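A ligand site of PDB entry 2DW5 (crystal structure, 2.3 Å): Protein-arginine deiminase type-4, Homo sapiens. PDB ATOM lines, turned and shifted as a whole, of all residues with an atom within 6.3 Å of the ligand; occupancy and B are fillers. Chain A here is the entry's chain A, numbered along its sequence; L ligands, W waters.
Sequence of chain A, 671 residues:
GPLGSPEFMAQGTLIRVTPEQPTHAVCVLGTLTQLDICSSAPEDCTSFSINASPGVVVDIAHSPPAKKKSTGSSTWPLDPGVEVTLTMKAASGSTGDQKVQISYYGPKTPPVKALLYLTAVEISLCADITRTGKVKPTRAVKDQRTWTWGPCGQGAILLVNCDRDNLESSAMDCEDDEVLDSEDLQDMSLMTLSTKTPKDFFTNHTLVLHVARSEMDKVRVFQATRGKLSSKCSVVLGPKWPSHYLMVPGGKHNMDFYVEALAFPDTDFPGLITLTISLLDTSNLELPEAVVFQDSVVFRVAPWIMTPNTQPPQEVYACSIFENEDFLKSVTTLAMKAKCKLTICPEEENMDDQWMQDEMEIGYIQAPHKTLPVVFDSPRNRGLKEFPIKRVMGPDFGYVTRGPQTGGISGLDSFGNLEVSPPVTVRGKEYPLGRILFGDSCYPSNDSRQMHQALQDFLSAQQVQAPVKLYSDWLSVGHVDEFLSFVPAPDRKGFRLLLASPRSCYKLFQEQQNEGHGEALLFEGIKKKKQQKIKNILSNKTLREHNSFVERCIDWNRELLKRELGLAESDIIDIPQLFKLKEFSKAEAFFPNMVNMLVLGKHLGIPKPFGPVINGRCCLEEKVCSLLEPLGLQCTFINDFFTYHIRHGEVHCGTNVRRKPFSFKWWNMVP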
ATOM      1  N   TRP A 355     -25.181 -25.361  12.638  1.00  0.00           N
ATOM      2  CA  TRP A 355     -25.954 -24.795  13.776  1.00  0.00           C
ATOM      3  C   TRP A 355     -27.340 -24.309  13.381  1.00  0.00           C
ATOM      4  O   TRP A 355     -27.626 -23.103  13.395  1.00  0.00           O
ATOM      5  CB  TRP A 355     -25.162 -23.713  14.490  1.00  0.00           C
ATOM      6  CG  TRP A 355     -23.783 -24.193  14.835  1.00  0.00           C
ATOM      7  CD1 TRP A 355     -22.599 -23.793  14.279  1.00  0.00           C
ATOM      8  CD2 TRP A 355     -23.479 -25.223  15.780  1.00  0.00           C
ATOM      9  NE1 TRP A 355     -21.563 -24.495  14.853  1.00  0.00           N
ATOM     10  CE2 TRP A 355     -22.065 -25.379  15.766  1.00  0.00           C
ATOM     11  CE3 TRP A 355     -24.230 -26.014  16.634  1.00  0.00           C
ATOM     12  CZ2 TRP A 355     -21.401 -26.312  16.596  1.00  0.00           C
ATOM     13  CZ3 TRP A 355     -23.574 -26.944  17.458  1.00  0.00           C
ATOM     14  CH2 TRP A 355     -22.179 -27.073  17.431  1.00  0.00           C
ATOM     15  N   GLN A 357     -30.116 -24.405  14.788  1.00  0.00           N
ATOM     16  CA  GLN A 357     -30.797 -23.607  15.819  1.00  0.00           C
ATOM     17  C   GLN A 357     -30.647 -22.090  15.635  1.00  0.00           C
ATOM     18  O   GLN A 357     -31.498 -21.308  16.077  1.00  0.00           O
ATOM     19  CB  GLN A 357     -30.238 -23.967  17.192  1.00  0.00           C
ATOM     20  CG  GLN A 357     -30.778 -23.129  18.380  1.00  0.00           C
ATOM     21  CD  GLN A 357     -32.264 -23.375  18.652  1.00  0.00           C
ATOM     22  OE1 GLN A 357     -32.937 -22.501  19.156  1.00  0.00           O
ATOM     23  NE2 GLN A 357     -32.771 -24.559  18.292  1.00  0.00           N
ATOM     24  N   ASP A 358     -29.562 -21.670  15.011  1.00  0.00           N
ATOM     25  CA  ASP A 358     -29.061 -20.326  15.217  1.00  0.00           C
ATOM     26  C   ASP A 358     -29.394 -19.261  14.148  1.00  0.00           C
ATOM     27  O   ASP A 358     -29.440 -18.072  14.493  1.00  0.00           O
ATOM     28  CB  ASP A 358     -27.546 -20.432  15.467  1.00  0.00           C
ATOM     29  CG  ASP A 358     -27.202 -21.032  16.846  1.00  0.00           C
ATOM     30  OD1 ASP A 358     -28.042 -20.978  17.791  1.00  0.00           O
ATOM     31  OD2 ASP A 358     -26.070 -21.529  16.990  1.00  0.00           O
ATOM     32  N   ARG A 380     -27.275 -13.236  11.796  1.00  0.00           N
ATOM     33  CA  ARG A 380     -25.945 -13.825  11.916  1.00  0.00           C
ATOM     34  C   ARG A 380     -25.351 -14.243  10.574  1.00  0.00           C
ATOM     35  O   ARG A 380     -24.128 -14.240  10.420  1.00  0.00           O
ATOM     36  CB  ARG A 380     -25.894 -14.958  12.938  1.00  0.00           C
ATOM     37  CG  ARG A 380     -26.392 -16.297  12.502  1.00  0.00           C
ATOM     38  CD  ARG A 380     -25.589 -17.415  13.163  1.00  0.00           C
ATOM     39  NE  ARG A 380     -26.008 -18.688  12.579  1.00  0.00           N
ATOM     40  CZ  ARG A 380     -25.292 -19.796  12.495  1.00  0.00           C
ATOM     41  NH1 ARG A 380     -24.069 -19.895  12.972  1.00  0.00           N
ATOM     42  NH2 ARG A 380     -25.845 -20.848  11.920  1.00  0.00           N
ATOM     43  N   ARG A 382     -24.477 -16.699   8.654  1.00  0.00           N
ATOM     44  CA  ARG A 382     -23.404 -17.664   8.538  1.00  0.00           C
ATOM     45  C   ARG A 382     -23.698 -18.548   7.295  1.00  0.00           C
ATOM     46  O   ARG A 382     -24.412 -18.122   6.379  1.00  0.00           O
ATOM     47  CB  ARG A 382     -23.366 -18.459   9.841  1.00  0.00           C
ATOM     48  CG  ARG A 382     -21.997 -18.719  10.352  1.00  0.00           C
ATOM     49  CD  ARG A 382     -21.440 -17.568  11.164  1.00  0.00           C
ATOM     50  NE  ARG A 382     -21.562 -17.753  12.611  1.00  0.00           N
ATOM     51  CZ  ARG A 382     -21.010 -18.729  13.344  1.00  0.00           C
ATOM     52  NH1 ARG A 382     -20.310 -19.716  12.793  1.00  0.00           N
ATOM     53  NH2 ARG A 382     -21.180 -18.732  14.645  1.00  0.00           N
ATOM     54  N   SER A 414     -27.599 -14.964  17.580  1.00  0.00           N
ATOM     55  CA  SER A 414     -27.957 -16.317  17.155  1.00  0.00           C
ATOM     56  C   SER A 414     -29.169 -16.780  17.958  1.00  0.00           C
ATOM     57  O   SER A 414     -29.306 -16.484  19.154  1.00  0.00           O
ATOM     58  CB  SER A 414     -26.780 -17.297  17.304  1.00  0.00           C
ATOM     59  OG  SER A 414     -25.655 -16.867  16.520  1.00  0.00           O
ATOM     60  N   PHE A 415     -30.068 -17.488  17.292  1.00  0.00           N
ATOM     61  CA  PHE A 415     -31.404 -17.700  17.830  1.00  0.00           C
ATOM     62  C   PHE A 415     -31.493 -18.879  18.738  1.00  0.00           C
ATOM     63  O   PHE A 415     -32.553 -19.191  19.227  1.00  0.00           O
ATOM     64  CB  PHE A 415     -32.438 -17.741  16.706  1.00  0.00           C
ATOM     65  CG  PHE A 415     -32.782 -16.361  16.137  1.00  0.00           C
ATOM     66  CD1 PHE A 415     -33.662 -16.246  15.082  1.00  0.00           C
ATOM     67  CD2 PHE A 415     -32.208 -15.191  16.648  1.00  0.00           C
ATOM     68  CE1 PHE A 415     -34.001 -15.017  14.550  1.00  0.00           C
ATOM     69  CE2 PHE A 415     -32.524 -13.942  16.115  1.00  0.00           C
ATOM     70  CZ  PHE A 415     -33.436 -13.873  15.075  1.00  0.00           C
ATOM     71  N   GLY A 416     -30.343 -19.478  19.049  1.00  0.00           N
ATOM     72  CA  GLY A 416     -30.193 -20.262  20.266  1.00  0.00           C
ATOM     73  C   GLY A 416     -30.282 -19.371  21.481  1.00  0.00           C
ATOM     74  O   GLY A 416     -30.568 -19.862  22.590  1.00  0.00           O
ATOM     75  N   ASN A 417     -30.034 -18.069  21.282  1.00  0.00           N
ATOM     76  CA  ASN A 417     -30.247 -17.067  22.325  1.00  0.00           C
ATOM     77  C   ASN A 417     -31.668 -16.478  22.317  1.00  0.00           C
ATOM     78  O   ASN A 417     -31.926 -15.520  23.039  1.00  0.00           O
ATOM     79  CB  ASN A 417     -29.213 -15.907  22.243  1.00  0.00           C
ATOM     80  CG  ASN A 417     -29.136 -15.103  23.547  1.00  0.00           C
ATOM     81  OD1 ASN A 417     -29.285 -15.674  24.644  1.00  0.00           O
ATOM     82  ND2 ASN A 417     -28.984 -13.784  23.444  1.00  0.00           N
ATOM     83  N   VAL A 477     -20.313 -19.000  24.246  1.00  0.00           N
ATOM     84  CA  VAL A 477     -21.219 -18.818  23.125  1.00  0.00           C
ATOM     85  C   VAL A 477     -22.288 -17.787  23.511  1.00  0.00           C
ATOM     86  O   VAL A 477     -22.580 -16.846  22.789  1.00  0.00           O
ATOM     87  CB  VAL A 477     -21.831 -20.172  22.729  1.00  0.00           C
ATOM     88  CG1 VAL A 477     -22.989 -20.005  21.737  1.00  0.00           C
ATOM     89  CG2 VAL A 477     -20.723 -21.119  22.186  1.00  0.00           C
ATOM     90  N   HIS A 479     -25.682 -18.330  24.963  1.00  0.00           N
ATOM     91  CA  HIS A 479     -27.128 -18.529  24.630  1.00  0.00           C
ATOM     92  C   HIS A 479     -27.925 -19.055  25.771  1.00  0.00           C
ATOM     93  O   HIS A 479     -27.435 -19.898  26.534  1.00  0.00           O
ATOM     94  CB  HIS A 479     -27.305 -19.502  23.469  1.00  0.00           C
ATOM     95  CG  HIS A 479     -26.622 -19.066  22.214  1.00  0.00           C
ATOM     96  ND1 HIS A 479     -26.546 -19.863  21.099  1.00  0.00           N
ATOM     97  CD2 HIS A 479     -25.941 -17.924  21.923  1.00  0.00           C
ATOM     98  CE1 HIS A 479     -25.836 -19.244  20.170  1.00  0.00           C
ATOM     99  NE2 HIS A 479     -25.468 -18.054  20.636  1.00  0.00           N
ATOM    100  N   ASP A 481     -30.147 -21.159  25.748  1.00  0.00           N
ATOM    101  CA  ASP A 481     -30.399 -22.610  25.581  1.00  0.00           C
ATOM    102  C   ASP A 481     -29.251 -23.422  26.170  1.00  0.00           C
ATOM    103  O   ASP A 481     -29.401 -24.575  26.466  1.00  0.00           O
ATOM    104  CB  ASP A 481     -30.819 -22.995  24.122  1.00  0.00           C
ATOM    105  CG  ASP A 481     -29.650 -22.978  23.082  1.00  0.00           C
ATOM    106  OD1 ASP A 481     -29.870 -23.543  21.943  1.00  0.00           O
ATOM    107  OD2 ASP A 481     -28.542 -22.414  23.355  1.00  0.00           O
ATOM    108  N   GLU A 482     -28.103 -22.783  26.401  1.00  0.00           N
ATOM    109  CA  GLU A 482     -27.027 -23.443  27.117  1.00  0.00           C
ATOM    110  C   GLU A 482     -27.276 -23.726  28.568  1.00  0.00           C
ATOM    111  O   GLU A 482     -26.561 -24.548  29.159  1.00  0.00           O
ATOM    112  CB  GLU A 482     -25.748 -22.636  26.987  1.00  0.00           C
ATOM    113  CG  GLU A 482     -25.296 -22.522  25.583  1.00  0.00           C
ATOM    114  CD  GLU A 482     -23.988 -21.814  25.487  1.00  0.00           C
ATOM    115  OE1 GLU A 482     -22.949 -22.510  25.553  1.00  0.00           O
ATOM    116  OE2 GLU A 482     -23.996 -20.564  25.404  1.00  0.00           O
ATOM    117  N   ASN A 596     -29.330 -28.839  26.873  1.00  0.00           N
ATOM    118  CA  ASN A 596     -29.420 -28.367  25.502  1.00  0.00           C
ATOM    119  C   ASN A 596     -29.929 -29.515  24.639  1.00  0.00           C
ATOM    120  O   ASN A 596     -29.227 -30.067  23.782  1.00  0.00           O
ATOM    121  CB  ASN A 596     -28.040 -27.848  25.078  1.00  0.00           C
ATOM    122  CG  ASN A 596     -28.042 -27.237  23.718  1.00  0.00           C
ATOM    123  OD1 ASN A 596     -27.957 -27.940  22.696  1.00  0.00           O
ATOM    124  ND2 ASN A 596     -28.158 -25.923  23.687  1.00  0.00           N
ATOM    125  N   ILE A 646     -17.556 -30.761  20.590  1.00  0.00           N
ATOM    126  CA  ILE A 646     -16.182 -30.220  20.443  1.00  0.00           C
ATOM    127  C   ILE A 646     -16.115 -28.899  19.681  1.00  0.00           C
ATOM    128  O   ILE A 646     -15.114 -28.183  19.782  1.00  0.00           O
ATOM    129  CB  ILE A 646     -15.189 -31.265  19.843  1.00  0.00           C
ATOM    130  CG1 ILE A 646     -15.627 -31.715  18.421  1.00  0.00           C
ATOM    131  CG2 ILE A 646     -15.051 -32.459  20.806  1.00  0.00           C
ATOM    132  CD1 ILE A 646     -14.660 -32.697  17.767  1.00  0.00           C
ATOM    133  N   ARG A 647     -17.186 -28.566  18.957  1.00  0.00           N
ATOM    134  CA  ARG A 647     -17.341 -27.220  18.383  1.00  0.00           C
ATOM    135  C   ARG A 647     -18.325 -26.325  19.171  1.00  0.00           C
ATOM    136  O   ARG A 647     -18.963 -25.409  18.597  1.00  0.00           O
ATOM    137  CB  ARG A 647     -17.720 -27.313  16.898  1.00  0.00           C
ATOM    138  CG  ARG A 647     -16.545 -27.793  16.038  1.00  0.00           C
ATOM    139  CD  ARG A 647     -16.958 -28.842  15.052  1.00  0.00           C
ATOM    140  NE  ARG A 647     -17.148 -28.280  13.720  1.00  0.00           N
ATOM    141  CZ  ARG A 647     -17.000 -28.967  12.576  1.00  0.00           C
ATOM    142  NH1 ARG A 647     -16.676 -30.259  12.622  1.00  0.00           N
ATOM    143  NH2 ARG A 647     -17.176 -28.355  11.403  1.00  0.00           N
ATOM    144  N   HIS A 648     -18.437 -26.619  20.469  1.00  0.00           N
ATOM    145  CA  HIS A 648     -19.055 -25.703  21.451  1.00  0.00           C
ATOM    146  C   HIS A 648     -20.592 -25.676  21.406  1.00  0.00           C
ATOM    147  O   HIS A 648     -21.197 -24.683  21.764  1.00  0.00           O
ATOM    148  CB  HIS A 648     -18.478 -24.274  21.304  1.00  0.00           C
ATOM    149  CG  HIS A 648     -17.005 -24.174  21.551  1.00  0.00           C
ATOM    150  ND1 HIS A 648     -16.131 -25.218  21.340  1.00  0.00           N
ATOM    151  CD2 HIS A 648     -16.244 -23.146  21.999  1.00  0.00           C
ATOM    152  CE1 HIS A 648     -14.901 -24.849  21.657  1.00  0.00           C
ATOM    153  NE2 HIS A 648     -14.941 -23.594  22.055  1.00  0.00           N
ATOM    154  N   GLY A 649     -21.215 -26.770  20.995  1.00  0.00           N
ATOM    155  CA  GLY A 649     -22.675 -26.862  20.968  1.00  0.00           C
ATOM    156  C   GLY A 649     -23.154 -28.293  21.040  1.00  0.00           C
ATOM    157  O   GLY A 649     -22.360 -29.215  21.013  1.00  0.00           O
ATOM    158  N   GLU A 650     -24.464 -28.480  21.070  1.00  0.00           N
ATOM    159  CA  GLU A 650     -25.069 -29.764  21.417  1.00  0.00           C
ATOM    160  C   GLU A 650     -26.241 -30.007  20.448  1.00  0.00           C
ATOM    161  O   GLU A 650     -26.299 -29.370  19.389  1.00  0.00           O
ATOM    162  CB  GLU A 650     -25.555 -29.669  22.871  1.00  0.00           C
ATOM    163  CG  GLU A 650     -24.769 -30.354  23.997  1.00  0.00           C
ATOM    164  CD  GLU A 650     -23.258 -30.498  23.837  1.00  0.00           C
ATOM    165  OE1 GLU A 650     -22.521 -29.809  24.564  1.00  0.00           O
ATOM    166  OE2 GLU A 650     -22.804 -31.396  23.085  1.00  0.00           O
ATOM    167  N   HIS A 652     -29.700 -29.453  20.679  1.00  0.00           N
ATOM    168  CA  HIS A 652     -30.591 -28.311  20.460  1.00  0.00           C
ATOM    169  C   HIS A 652     -29.930 -27.354  19.483  1.00  0.00           C
ATOM    170  O   HIS A 652     -30.551 -26.900  18.525  1.00  0.00           O
ATOM    171  CB  HIS A 652     -30.895 -27.592  21.787  1.00  0.00           C
ATOM    172  CG  HIS A 652     -32.058 -26.645  21.731  1.00  0.00           C
ATOM    173  ND1 HIS A 652     -31.905 -25.284  21.538  1.00  0.00           N
ATOM    174  CD2 HIS A 652     -33.389 -26.856  21.836  1.00  0.00           C
ATOM    175  CE1 HIS A 652     -33.091 -24.695  21.538  1.00  0.00           C
ATOM    176  NE2 HIS A 652     -34.017 -25.628  21.707  1.00  0.00           N
ATOM    177  N   CYS A 653     -28.657 -27.052  19.710  1.00  0.00           N
ATOM    178  CA  CYS A 653     -27.914 -26.157  18.802  1.00  0.00           C
ATOM    179  C   CYS A 653     -27.859 -26.640  17.339  1.00  0.00           C
ATOM    180  O   CYS A 653     -27.766 -25.821  16.426  1.00  0.00           O
ATOM    181  CB  CYS A 653     -26.479 -25.961  19.299  1.00  0.00           C
ATOM    182  SG  CYS A 653     -26.375 -25.630  21.045  1.00  0.00           S
ATOM    183  N   GLY A 654     -27.847 -27.963  17.142  1.00  0.00           N
ATOM    184  CA  GLY A 654     -27.833 -28.559  15.798  1.00  0.00           C
ATOM    185  C   GLY A 654     -29.200 -28.742  15.126  1.00  0.00           C
ATOM    186  O   GLY A 654     -29.264 -29.192  13.960  1.00  0.00           O
HETATM  187  O1  LIG L   1     -21.829 -20.191  17.094  1.00  0.00           O
HETATM  188  C1  LIG L   1     -20.935 -20.847  17.564  1.00  0.00           C
HETATM  189  N1  LIG L   1     -20.017 -20.346  18.398  1.00  0.00           N
HETATM  190  C2  LIG L   1     -20.879 -22.287  17.177  1.00  0.00           C
HETATM  191  C3  LIG L   1     -21.460 -23.159  18.288  1.00  0.00           C
HETATM  192  C4  LIG L   1     -22.547 -22.550  19.156  1.00  0.00           C
HETATM  193  C5  LIG L   1     -23.953 -22.493  18.567  1.00  0.00           C
HETATM  194  N2  LIG L   1     -24.723 -23.114  19.638  1.00  0.00           N
HETATM  195  C6  LIG L   1     -25.917 -23.137  20.242  1.00  0.00           C
HETATM  196  C7  LIG L   1     -25.743 -24.155  21.333  1.00  0.00           C
HETATM  197  N3  LIG L   1     -27.065 -22.519  19.968  1.00  0.00           N
HETATM  198  N4  LIG L   1     -19.516 -22.802  16.926  1.00  0.00           N
HETATM  199  C8  LIG L   1     -18.639 -22.247  16.080  1.00  0.00           C
HETATM  200  O2  LIG L   1     -18.925 -21.249  15.437  1.00  0.00           O
HETATM  201  C9  LIG L   1     -17.274 -22.868  15.919  1.00  0.00           C
HETATM  202  C10 LIG L   1     -16.795 -23.826  16.830  1.00  0.00           C
HETATM  203  C11 LIG L   1     -16.436 -22.498  14.851  1.00  0.00           C
HETATM  204  C12 LIG L   1     -15.167 -23.074  14.705  1.00  0.00           C
HETATM  205  C13 LIG L   1     -14.715 -24.021  15.620  1.00  0.00           C
HETATM  206  C14 LIG L   1     -15.526 -24.402  16.684  1.00  0.00           C
HETATM  207  O   HOH W   1     -23.968 -20.407  15.616  1.00  0.00           O
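The side-chain sulfur (SG) of Cys 653 is covalently linked to a carbon (C7) of the ligand (1.6 Å).
The side-chain carboxylate (OD1) of Asp 358 lies within salt-bridge range of a nitrogen (N3) of the ligand, 2.8 Å away.
O1 of the ligand sits at hydrogen-bond distance from NH2 of Arg 382 (2.9 Å).
N3 of the ligand is in hydrogen-bond range of ND1 of His 479, 2.9 Å away.
The backbone carbonyl oxygen of Arg 647 sits at hydrogen-bond distance from a nitrogen (N4) of the ligand, at 3.1 Å.
The side-chain carboxylate of Asp 481 is in salt-bridge range of a nitrogen (N3) of the ligand (3.6 Å).
N of Gln 357 lies close to O of Cys 653 (3.2 Å).
The backbone NH (N) of Glu 650 lies within hydrogen-bond range of the side-chain sulfur (SG) of Cys 653, at 3.4 Å.
The backbone NH (N) of Gly 416 is in hydrogen-bond range of the side-chain carboxylate (OD1) of Asp 358, 3.0 Å away.
The side-chain carboxylate of Glu 482 sits at hydrogen-bond distance from the backbone NH of His 479, 2.8 Å away.
NH2 of Arg 380 is in hydrogen-bond range of O of Trp 355, 3.2 Å away.
The backbone carbonyl oxygen (O) of Gly 416 sits close to the backbone NH (N) of Asp 481 (3.4 Å).
ND1 of His 652 lies within hydrogen-bond range of OD1 of Asp 481.
The backbone NH of His 652 sits at hydrogen-bond distance from the side-chain amide oxygen of Asn 596 (3.1 Å).
The indole nitrogen (NE1) of Trp 355 lies close to a nitrogen (N4) of the ligand (3.4 Å).
Gly 416 touches the ligand.
Val 477 touches the ligand (CG1 to C4, 3.7 Å).
Asn 596 touches the ligand.
O of His 648 touches C4 of the ligand (3.6 Å).
11 residues have an atom within 4 Å of the ligand: Trp 355, Asp 358, Arg 382, Gly 416, Val 477, His 479, Asp 481, Asn 596, Arg 647, His 648 and Cys 653.
The nearest printed residue that does not touch the ligand is Gln 357 (4.1 Å).
Water W1 lies within hydrogen-bond range of O1 of the ligand, NH1 of Arg 380, OD2 of Asp 358 and NH2 of Arg 382.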
